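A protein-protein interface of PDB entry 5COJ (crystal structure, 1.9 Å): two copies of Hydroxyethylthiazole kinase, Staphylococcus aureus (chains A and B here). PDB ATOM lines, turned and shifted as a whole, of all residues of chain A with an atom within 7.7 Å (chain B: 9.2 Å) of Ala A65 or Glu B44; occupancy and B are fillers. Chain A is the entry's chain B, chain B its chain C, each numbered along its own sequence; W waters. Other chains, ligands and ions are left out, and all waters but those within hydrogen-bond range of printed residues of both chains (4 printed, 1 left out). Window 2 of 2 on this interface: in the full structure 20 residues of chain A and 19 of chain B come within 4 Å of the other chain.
Of the printed residues of chain B, Leu A63 touches Ala B42 (3.5 Å). Of chain B, only Glu B41 (3.97 Å) and Ala B42 (3.96 Å) come within 4 Å of Thr A64. No residue of chain B comes within 4 Å of Gln A66. Asp A70 touches none of the printed residues of chain B. Of the printed residues of chain B, Tyr A97 touches Ala B42 (3.6 Å), Glu B44 (3.6 Å) and Glu B45 (3.8 Å). Printed residues of chain A within 4 Å of Glu B41: Thr A64. Of the printed residues of chain A, Ala B42 touches Leu A63 (3.5 Å), Thr A64 (3.96 Å) and Tyr A97 (3.6 Å). Of chain A, only Ala A65 (3.96 Å) and Tyr A97 (3.6 Å) come within 4 Å of Glu B44. Of the printed residues of chain A, Glu B45 touches Ser A95 (2.7 Å), Tyr A97 (3.8 Å) and Arg A98 (2.7 Å). The nearest residue of chain B that does not touch Ala A65 is Ala B42 (5.3 Å). The nearest printed residue of chain A that does not touch Glu B45 is Leu A63 (4.7 Å).
2 positions are printed for both chains.
The side-chain hydroxyl of Ser A95 lies within hydrogen-bond range of the side-chain carboxylate of Glu B45. N of Thr A96 sits at hydrogen-bond distance from OE1 of Glu B48, at 2.8 Å. The side-chain carboxylate (OE1) of Glu B45 is in salt-bridge range of the guanidinium group (NE) of Arg A98 (2.7 Å).
Water W3 lies within hydrogen-bond range of OD2 of Asp B70 and NE2 of Gln A66. Water W4 lies within hydrogen-bond range of O of Leu A63 (2.7 Å), OE2 of Glu B45 (2.9 Å), N of Glu B41 (3.1 Å) and N of Ala B42 (3.2 Å). Water W2 bridges OE2 of Glu A68 (2.8 Å) and OE2 of Glu B44 (2.9 Å). Water W1 bridges OE1 of Glu B44 (2.8 Å) and N of Ala A65 (2.9 Å).
Printed residues of chain B that touch a printed residue of chain A: Glu B41, Ala B42, Glu B44, Glu B45 and Glu B48.
O of Leu A63 touches CB of Ala B42, 3.5 Å away. CB of Glu B41 touches CG2 of Thr A64, 3.97 Å away. Ala B42 touches Thr A64 (N to CG2, 3.96 Å). Ala A65 touches Glu B44 (CB to OE2, 3.96 Å). OE1 of Glu B48 touches CB of Ser A95 (3.4 Å). CE2 of Tyr A97 touches CB of Ala B42, 3.6 Å away. Tyr A97 touches Glu B44. Tyr A97 touches Glu B45 (CD2 to OE1, 3.8 Å).
The backbone NH (N) of Thr A64 lies within hydrogen-bond range of the side-chain amide oxygen (OD1) of Asn A67, at 3.1 Å. N of Ala A65 sits at hydrogen-bond distance from OH of Tyr A97 (3.3 Å). OE2 of Glu A68 lies within hydrogen-bond range of OH of Tyr A97 (2.6 Å). OG of Ser A95 is in hydrogen-bond range of N of Arg A98 (3.2 Å). The side-chain carboxylate (OE2) of Glu B45 is in hydrogen-bond range of the side-chain hydroxyl (OG) of Ser B40 (2.6 Å).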
ATOM      1  N   THR A  62       6.525 -21.839  12.248  1.00  0.00           N
ATOM      2  CA  THR A  62       7.789 -21.977  11.454  1.00  0.00           C
ATOM      3  C   THR A  62       7.531 -21.534  10.030  1.00  0.00           C
ATOM      4  O   THR A  62       8.041 -22.097   9.093  1.00  0.00           O
ATOM      5  CB  THR A  62       8.379 -23.454  11.551  1.00  0.00           C
ATOM      6  OG1 THR A  62       7.338 -24.434  11.330  1.00  0.00           O
ATOM      7  CG2 THR A  62       8.970 -23.738  12.933  1.00  0.00           C
ATOM      8  N   LEU A  63       6.872 -20.393   9.885  1.00  0.00           N
ATOM      9  CA  LEU A  63       6.549 -19.829   8.594  1.00  0.00           C
ATOM     10  C   LEU A  63       7.796 -19.614   7.733  1.00  0.00           C
ATOM     11  O   LEU A  63       8.773 -19.009   8.206  1.00  0.00           O
ATOM     12  CB  LEU A  63       5.864 -18.453   8.767  1.00  0.00           C
ATOM     13  CG  LEU A  63       5.425 -17.753   7.519  1.00  0.00           C
ATOM     14  CD1 LEU A  63       4.241 -18.502   6.924  1.00  0.00           C
ATOM     15  CD2 LEU A  63       4.994 -16.342   7.887  1.00  0.00           C
ATOM     16  N   THR A  64       7.754 -20.125   6.487  1.00  0.00           N
ATOM     17  CA  THR A  64       8.798 -19.830   5.450  1.00  0.00           C
ATOM     18  C   THR A  64       8.139 -19.619   4.101  1.00  0.00           C
ATOM     19  O   THR A  64       6.906 -19.802   3.930  1.00  0.00           O
ATOM     20  CB  THR A  64       9.813 -20.996   5.317  1.00  0.00           C
ATOM     21  OG1 THR A  64       9.164 -22.208   4.888  1.00  0.00           O
ATOM     22  CG2 THR A  64      10.502 -21.329   6.626  1.00  0.00           C
ATOM     23  N   ALA A  65       8.911 -19.163   3.132  1.00  0.00           N
ATOM     24  CA  ALA A  65       8.402 -18.957   1.767  1.00  0.00           C
ATOM     25  C   ALA A  65       7.722 -20.182   1.166  1.00  0.00           C
ATOM     26  O   ALA A  65       6.692 -20.041   0.509  1.00  0.00           O
ATOM     27  CB  ALA A  65       9.515 -18.510   0.859  1.00  0.00           C
ATOM     28  N   GLN A  66       8.156 -21.380   1.541  1.00  0.00           N
ATOM     29  CA  GLN A  66       7.474 -22.608   1.132  1.00  0.00           C
ATOM     30  C   GLN A  66       6.009 -22.741   1.586  1.00  0.00           C
ATOM     31  O   GLN A  66       5.244 -23.445   0.954  1.00  0.00           O
ATOM     32  CB  GLN A  66       8.257 -23.820   1.653  1.00  0.00           C
ATOM     33  CG  GLN A  66       9.470 -24.212   0.802  1.00  0.00           C
ATOM     34  CD  GLN A  66      10.412 -23.046   0.421  1.00  0.00           C
ATOM     35  OE1 GLN A  66      10.408 -22.552  -0.713  1.00  0.00           O
ATOM     36  NE2 GLN A  66      11.233 -22.624   1.381  1.00  0.00           N
ATOM     37  N   ASN A  67       5.647 -22.133   2.716  1.00  0.00           N
ATOM     38  CA  ASN A  67       4.315 -22.198   3.269  1.00  0.00           C
ATOM     39  C   ASN A  67       3.403 -21.076   2.829  1.00  0.00           C
ATOM     40  O   ASN A  67       2.219 -21.227   2.893  1.00  0.00           O
ATOM     41  CB  ASN A  67       4.341 -22.065   4.802  1.00  0.00           C
ATOM     42  CG  ASN A  67       5.206 -23.085   5.489  1.00  0.00           C
ATOM     43  OD1 ASN A  67       6.053 -22.736   6.268  1.00  0.00           O
ATOM     44  ND2 ASN A  67       4.904 -24.349   5.291  1.00  0.00           N
ATOM     45  N   GLU A  68       3.943 -19.889   2.492  1.00  0.00           N
ATOM     46  CA  GLU A  68       3.088 -18.700   2.433  1.00  0.00           C
ATOM     47  C   GLU A  68       1.895 -18.852   1.477  1.00  0.00           C
ATOM     48  O   GLU A  68       0.742 -18.665   1.883  1.00  0.00           O
ATOM     49  CB  GLU A  68       3.846 -17.424   2.004  1.00  0.00           C
ATOM     50  CG  GLU A  68       4.803 -16.926   3.066  1.00  0.00           C
ATOM     51  CD  GLU A  68       5.767 -15.887   2.490  1.00  0.00           C
ATOM     52  OE1 GLU A  68       5.273 -14.958   1.874  1.00  0.00           O
ATOM     53  OE2 GLU A  68       7.006 -16.055   2.651  1.00  0.00           O
ATOM     54  N   GLN A  69       2.181 -19.075   0.193  1.00  0.00           N
ATOM     55  CA  GLN A  69       1.086 -19.199  -0.763  1.00  0.00           C
ATOM     56  C   GLN A  69       0.104 -20.340  -0.429  1.00  0.00           C
ATOM     57  O   GLN A  69      -1.111 -20.199  -0.661  1.00  0.00           O
ATOM     58  CB  GLN A  69       1.595 -19.416  -2.176  1.00  0.00           C
ATOM     59  CG  GLN A  69       0.535 -19.314  -3.254  1.00  0.00           C
ATOM     60  CD  GLN A  69      -0.481 -18.201  -2.990  1.00  0.00           C
ATOM     61  OE1 GLN A  69      -0.097 -17.060  -3.039  1.00  0.00           O
ATOM     62  NE2 GLN A  69      -1.761 -18.524  -2.656  1.00  0.00           N
ATOM     63  N   ASP A  70       0.624 -21.462   0.040  1.00  0.00           N
ATOM     64  CA  ASP A  70      -0.203 -22.611   0.329  1.00  0.00           C
ATOM     65  C   ASP A  70      -1.197 -22.316   1.487  1.00  0.00           C
ATOM     66  O   ASP A  70      -2.355 -22.772   1.460  1.00  0.00           O
ATOM     67  CB  ASP A  70       0.679 -23.831   0.718  1.00  0.00           C
ATOM     68  CG  ASP A  70       1.396 -24.489  -0.486  1.00  0.00           C
ATOM     69  OD1 ASP A  70       1.146 -24.094  -1.611  1.00  0.00           O
ATOM     70  OD2 ASP A  70       2.221 -25.404  -0.262  1.00  0.00           O
ATOM     71  N   SER A  95       8.646 -10.110  13.967  1.00  0.00           N
ATOM     72  CA  SER A  95       9.196  -9.649  12.684  1.00  0.00           C
ATOM     73  C   SER A  95       8.178  -9.011  11.753  1.00  0.00           C
ATOM     74  O   SER A  95       6.971  -9.379  11.759  1.00  0.00           O
ATOM     75  CB  SER A  95       9.875 -10.844  11.959  1.00  0.00           C
ATOM     76  OG  SER A  95       8.923 -11.897  11.578  1.00  0.00           O
ATOM     77  N   THR A  96       8.648  -8.113  10.920  1.00  0.00           N
ATOM     78  CA  THR A  96       7.800  -7.532   9.902  1.00  0.00           C
ATOM     79  C   THR A  96       7.336  -8.587   8.867  1.00  0.00           C
ATOM     80  O   THR A  96       6.191  -8.531   8.394  1.00  0.00           O
ATOM     81  CB  THR A  96       8.505  -6.316   9.249  1.00  0.00           C
ATOM     82  OG1 THR A  96       9.727  -6.754   8.702  1.00  0.00           O
ATOM     83  CG2 THR A  96       8.837  -5.291  10.314  1.00  0.00           C
ATOM     84  N   TYR A  97       8.184  -9.594   8.604  1.00  0.00           N
ATOM     85  CA  TYR A  97       7.812 -10.784   7.827  1.00  0.00           C
ATOM     86  C   TYR A  97       6.487 -11.413   8.340  1.00  0.00           C
ATOM     87  O   TYR A  97       5.564 -11.650   7.573  1.00  0.00           O
ATOM     88  CB  TYR A  97       8.966 -11.815   7.854  1.00  0.00           C
ATOM     89  CG  TYR A  97       8.758 -13.098   7.086  1.00  0.00           C
ATOM     90  CD1 TYR A  97       8.438 -13.085   5.725  1.00  0.00           C
ATOM     91  CD2 TYR A  97       8.717 -14.316   7.751  1.00  0.00           C
ATOM     92  CE1 TYR A  97       8.178 -14.256   5.013  1.00  0.00           C
ATOM     93  CE2 TYR A  97       8.493 -15.510   7.063  1.00  0.00           C
ATOM     94  CZ  TYR A  97       8.215 -15.459   5.668  1.00  0.00           C
ATOM     95  OH  TYR A  97       7.969 -16.633   5.049  1.00  0.00           O
ATOM     96  N   ARG A  98       6.420 -11.741   9.613  1.00  0.00           N
ATOM     97  CA  ARG A  98       5.211 -12.325  10.161  1.00  0.00           C
ATOM     98  C   ARG A  98       4.031 -11.365  10.231  1.00  0.00           C
ATOM     99  O   ARG A  98       2.915 -11.754   9.942  1.00  0.00           O
ATOM    100  CB  ARG A  98       5.473 -12.909  11.552  1.00  0.00           C
ATOM    101  CG  ARG A  98       6.379 -14.110  11.548  1.00  0.00           C
ATOM    102  CD  ARG A  98       6.785 -14.519  12.963  1.00  0.00           C
ATOM    103  NE  ARG A  98       7.772 -15.566  12.877  1.00  0.00           N
ATOM    104  CZ  ARG A  98       7.512 -16.847  12.930  1.00  0.00           C
ATOM    105  NH1 ARG A  98       6.362 -17.243  13.386  1.00  0.00           N
ATOM    106  NH2 ARG A  98       8.493 -17.745  12.800  1.00  0.00           N
ATOM    107  N   GLN A 100       3.389  -8.830   8.209  1.00  0.00           N
ATOM    108  CA  GLN A 100       2.856  -8.686   6.863  1.00  0.00           C
ATOM    109  C   GLN A 100       2.053  -9.909   6.447  1.00  0.00           C
ATOM    110  O   GLN A 100       0.979  -9.770   5.845  1.00  0.00           O
ATOM    111  CB  GLN A 100       3.953  -8.407   5.825  1.00  0.00           C
ATOM    112  CG  GLN A 100       4.611  -7.079   5.983  1.00  0.00           C
ATOM    113  CD  GLN A 100       5.926  -6.950   5.061  1.00  0.00           C
ATOM    114  OE1 GLN A 100       6.601  -7.959   4.641  1.00  0.00           O
ATOM    115  NE2 GLN A 100       6.267  -5.731   4.771  1.00  0.00           N
ATOM    116  N   SER B  40      13.356 -20.615  14.004  1.00  0.00           N
ATOM    117  CA  SER B  40      13.113 -19.740  12.824  1.00  0.00           C
ATOM    118  C   SER B  40      13.991 -20.170  11.669  1.00  0.00           C
ATOM    119  O   SER B  40      15.213 -20.192  11.784  1.00  0.00           O
ATOM    120  CB  SER B  40      13.347 -18.286  13.220  1.00  0.00           C
ATOM    121  OG  SER B  40      13.239 -17.406  12.070  1.00  0.00           O
ATOM    122  N   GLU B  41      13.371 -20.432  10.517  1.00  0.00           N
ATOM    123  CA  GLU B  41      14.073 -20.844   9.329  1.00  0.00           C
ATOM    124  C   GLU B  41      13.968 -19.918   8.083  1.00  0.00           C
ATOM    125  O   GLU B  41      14.628 -20.206   7.091  1.00  0.00           O
ATOM    126  CB  GLU B  41      13.622 -22.221   8.909  1.00  0.00           C
ATOM    127  CG  GLU B  41      13.880 -23.246   9.965  1.00  0.00           C
ATOM    128  CD  GLU B  41      13.440 -24.667   9.596  1.00  0.00           C
ATOM    129  OE1 GLU B  41      13.151 -24.952   8.403  1.00  0.00           O
ATOM    130  OE2 GLU B  41      13.309 -25.492  10.561  1.00  0.00           O
ATOM    131  N   ALA B  42      13.179 -18.845   8.157  1.00  0.00           N
ATOM    132  CA  ALA B  42      12.966 -17.929   7.084  1.00  0.00           C
ATOM    133  C   ALA B  42      14.048 -16.850   7.066  1.00  0.00           C
ATOM    134  O   ALA B  42      14.215 -16.101   8.052  1.00  0.00           O
ATOM    135  CB  ALA B  42      11.627 -17.270   7.227  1.00  0.00           C
ATOM    136  N   PRO B  43      14.830 -16.776   5.985  1.00  0.00           N
ATOM    137  CA  PRO B  43      15.876 -15.752   5.970  1.00  0.00           C
ATOM    138  C   PRO B  43      15.286 -14.347   6.066  1.00  0.00           C
ATOM    139  O   PRO B  43      15.952 -13.436   6.497  1.00  0.00           O
ATOM    140  CB  PRO B  43      16.558 -15.930   4.583  1.00  0.00           C
ATOM    141  CG  PRO B  43      16.405 -17.383   4.321  1.00  0.00           C
ATOM    142  CD  PRO B  43      15.012 -17.767   4.929  1.00  0.00           C
ATOM    143  N   GLU B  44      14.063 -14.198   5.613  1.00  0.00           N
ATOM    144  CA  GLU B  44      13.371 -12.911   5.589  1.00  0.00           C
ATOM    145  C   GLU B  44      13.188 -12.320   7.019  1.00  0.00           C
ATOM    146  O   GLU B  44      12.981 -11.124   7.161  1.00  0.00           O
ATOM    147  CB  GLU B  44      11.963 -13.083   4.954  1.00  0.00           C
ATOM    148  CG  GLU B  44      11.970 -13.494   3.481  1.00  0.00           C
ATOM    149  CD  GLU B  44      11.966 -15.002   3.224  1.00  0.00           C
ATOM    150  OE1 GLU B  44      12.367 -15.823   4.101  1.00  0.00           O
ATOM    151  OE2 GLU B  44      11.618 -15.393   2.108  1.00  0.00           O
ATOM    152  N   GLU B  45      13.267 -13.125   8.070  1.00  0.00           N
ATOM    153  CA  GLU B  45      13.156 -12.582   9.435  1.00  0.00           C
ATOM    154  C   GLU B  45      14.430 -12.736  10.250  1.00  0.00           C
ATOM    155  O   GLU B  45      14.457 -12.432  11.451  1.00  0.00           O
ATOM    156  CB  GLU B  45      11.972 -13.215  10.220  1.00  0.00           C
ATOM    157  CG  GLU B  45      12.085 -14.684  10.522  1.00  0.00           C
ATOM    158  CD  GLU B  45      10.838 -15.233  11.280  1.00  0.00           C
ATOM    159  OE1 GLU B  45       9.831 -14.487  11.425  1.00  0.00           O
ATOM    160  OE2 GLU B  45      10.827 -16.438  11.602  1.00  0.00           O
ATOM    161  N   ALA B  46      15.498 -13.173   9.604  1.00  0.00           N
ATOM    162  CA  ALA B  46      16.758 -13.430  10.335  1.00  0.00           C
ATOM    163  C   ALA B  46      17.375 -12.164  10.896  1.00  0.00           C
ATOM    164  O   ALA B  46      17.798 -12.121  12.047  1.00  0.00           O
ATOM    165  CB  ALA B  46      17.750 -14.152   9.465  1.00  0.00           C
ATOM    166  N   GLU B  47      17.420 -11.101  10.102  1.00  0.00           N
ATOM    167  CA  GLU B  47      17.949  -9.862  10.610  1.00  0.00           C
ATOM    168  C   GLU B  47      17.285  -9.310  11.876  1.00  0.00           C
ATOM    169  O   GLU B  47      17.960  -8.940  12.813  1.00  0.00           O
ATOM    170  CB  GLU B  47      17.894  -8.806   9.507  1.00  0.00           C
ATOM    171  CG  GLU B  47      19.068  -7.938   9.501  1.00  0.00           C
ATOM    172  CD  GLU B  47      18.961  -6.886   8.420  1.00  0.00           C
ATOM    173  OE1 GLU B  47      19.091  -7.233   7.228  1.00  0.00           O
ATOM    174  OE2 GLU B  47      18.759  -5.717   8.788  1.00  0.00           O
ATOM    175  N   GLU B  48      15.951  -9.294  11.924  1.00  0.00           N
ATOM    176  CA  GLU B  48      15.229  -8.814  13.095  1.00  0.00           C
ATOM    177  C   GLU B  48      15.331  -9.776  14.271  1.00  0.00           C
ATOM    178  O   GLU B  48      15.452  -9.336  15.407  1.00  0.00           O
ATOM    179  CB  GLU B  48      13.737  -8.581  12.777  1.00  0.00           C
ATOM    180  CG  GLU B  48      13.492  -7.453  11.786  1.00  0.00           C
ATOM    181  CD  GLU B  48      11.994  -7.408  11.513  1.00  0.00           C
ATOM    182  OE1 GLU B  48      11.481  -8.129  10.621  1.00  0.00           O
ATOM    183  OE2 GLU B  48      11.341  -6.867  12.417  1.00  0.00           O
ATOM    184  N   PHE B  49      15.233 -11.065  14.038  1.00  0.00           N
ATOM    185  CA  PHE B  49      15.433 -12.014  15.145  1.00  0.00           C
ATOM    186  C   PHE B  49      16.838 -11.989  15.722  1.00  0.00           C
ATOM    187  O   PHE B  49      17.012 -12.088  16.931  1.00  0.00           O
ATOM    188  CB  PHE B  49      15.139 -13.467  14.685  1.00  0.00           C
ATOM    189  CG  PHE B  49      13.733 -13.922  14.954  1.00  0.00           C
ATOM    190  CD1 PHE B  49      12.694 -13.422  14.214  1.00  0.00           C
ATOM    191  CD2 PHE B  49      13.462 -14.903  15.881  1.00  0.00           C
ATOM    192  CE1 PHE B  49      11.368 -13.867  14.421  1.00  0.00           C
ATOM    193  CE2 PHE B  49      12.135 -15.320  16.134  1.00  0.00           C
ATOM    194  CZ  PHE B  49      11.111 -14.840  15.333  1.00  0.00           C
ATOM    195  N   TYR B  50      17.837 -11.869  14.859  1.00  0.00           N
ATOM    196  CA  TYR B  50      19.235 -12.079  15.283  1.00  0.00           C
ATOM    197  C   TYR B  50      19.760 -10.925  16.093  1.00  0.00           C
ATOM    198  O   TYR B  50      20.570 -11.112  17.014  1.00  0.00           O
ATOM    199  CB  TYR B  50      20.143 -12.321  14.100  1.00  0.00           C
ATOM    200  CG  TYR B  50      19.981 -13.676  13.423  1.00  0.00           C
ATOM    201  CD1 TYR B  50      18.969 -14.567  13.777  1.00  0.00           C
ATOM    202  CD2 TYR B  50      20.835 -14.039  12.400  1.00  0.00           C
ATOM    203  CE1 TYR B  50      18.834 -15.751  13.105  1.00  0.00           C
ATOM    204  CE2 TYR B  50      20.720 -15.229  11.760  1.00  0.00           C
ATOM    205  CZ  TYR B  50      19.715 -16.114  12.115  1.00  0.00           C
ATOM    206  OH  TYR B  50      19.578 -17.289  11.411  1.00  0.00           O
ATOM    207  N   GLN B  66      16.217 -27.603  -0.365  1.00  0.00           N
ATOM    208  CA  GLN B  66      15.374 -26.545   0.222  1.00  0.00           C
ATOM    209  C   GLN B  66      16.141 -25.741   1.295  1.00  0.00           C
ATOM    210  O   GLN B  66      15.796 -24.605   1.510  1.00  0.00           O
ATOM    211  CB  GLN B  66      14.010 -27.094   0.770  1.00  0.00           C
ATOM    212  CG  GLN B  66      13.583 -26.551   2.162  1.00  0.00           C
ATOM    213  CD  GLN B  66      12.499 -27.393   2.868  1.00  0.00           C
ATOM    214  OE1 GLN B  66      11.492 -27.741   2.255  1.00  0.00           O
ATOM    215  NE2 GLN B  66      12.717 -27.754   4.151  1.00  0.00           N
ATOM    216  N   ASP B  70      19.451 -21.131   1.965  1.00  0.00           N
ATOM    217  CA  ASP B  70      18.978 -20.448   3.152  1.00  0.00           C
ATOM    218  C   ASP B  70      19.997 -20.517   4.349  1.00  0.00           C
ATOM    219  O   ASP B  70      20.166 -19.526   5.073  1.00  0.00           O
ATOM    220  CB  ASP B  70      17.617 -21.033   3.624  1.00  0.00           C
ATOM    221  CG  ASP B  70      16.444 -20.677   2.708  1.00  0.00           C
ATOM    222  OD1 ASP B  70      16.638 -19.896   1.771  1.00  0.00           O
ATOM    223  OD2 ASP B  70      15.339 -21.168   2.918  1.00  0.00           O
ATOM    224  N   ALA B  73      22.793 -18.122   3.634  1.00  0.00           N
ATOM    225  CA  ALA B  73      22.303 -16.754   3.819  1.00  0.00           C
ATOM    226  C   ALA B  73      22.160 -16.362   5.275  1.00  0.00           C
ATOM    227  O   ALA B  73      22.650 -15.288   5.663  1.00  0.00           O
ATOM    228  CB  ALA B  73      20.980 -16.526   3.068  1.00  0.00           C
ATOM    229  N   ILE B  74      21.555 -17.235   6.133  1.00  0.00           N
ATOM    230  CA  ILE B  74      21.415 -16.895   7.510  1.00  0.00           C
ATOM    231  C   ILE B  74      22.748 -16.893   8.272  1.00  0.00           C
ATOM    232  O   ILE B  74      22.908 -16.166   9.262  1.00  0.00           O
ATOM    233  CB  ILE B  74      20.363 -17.755   8.289  1.00  0.00           C
ATOM    234  CG1 ILE B  74      20.840 -19.204   8.456  1.00  0.00           C
ATOM    235  CG2 ILE B  74      19.002 -17.623   7.625  1.00  0.00           C
ATOM    236  CD1 ILE B  74      19.963 -20.034   9.247  1.00  0.00           C
ATOM    237  N   THR B  77      24.032 -13.573   7.707  1.00  0.00           N
ATOM    238  CA  THR B  77      23.281 -12.623   8.494  1.00  0.00           C
ATOM    239  C   THR B  77      23.736 -12.652   9.933  1.00  0.00           C
ATOM    240  O   THR B  77      23.844 -11.620  10.582  1.00  0.00           O
ATOM    241  CB  THR B  77      21.758 -12.873   8.388  1.00  0.00           C
ATOM    242  OG1 THR B  77      21.349 -12.810   7.009  1.00  0.00           O
ATOM    243  CG2 THR B  77      20.982 -11.884   9.178  1.00  0.00           C
HETATM  244  O   HOH W   1      11.607 -18.488   4.040  1.00  0.00           O
HETATM  245  O   HOH W   2       8.928 -14.884   1.060  1.00  0.00           O
HETATM  246  O   HOH W   3      13.296 -19.916   2.054  1.00  0.00           O
HETATM  247  O   HOH W   4      10.701 -18.923  10.130  1.00  0.00           O
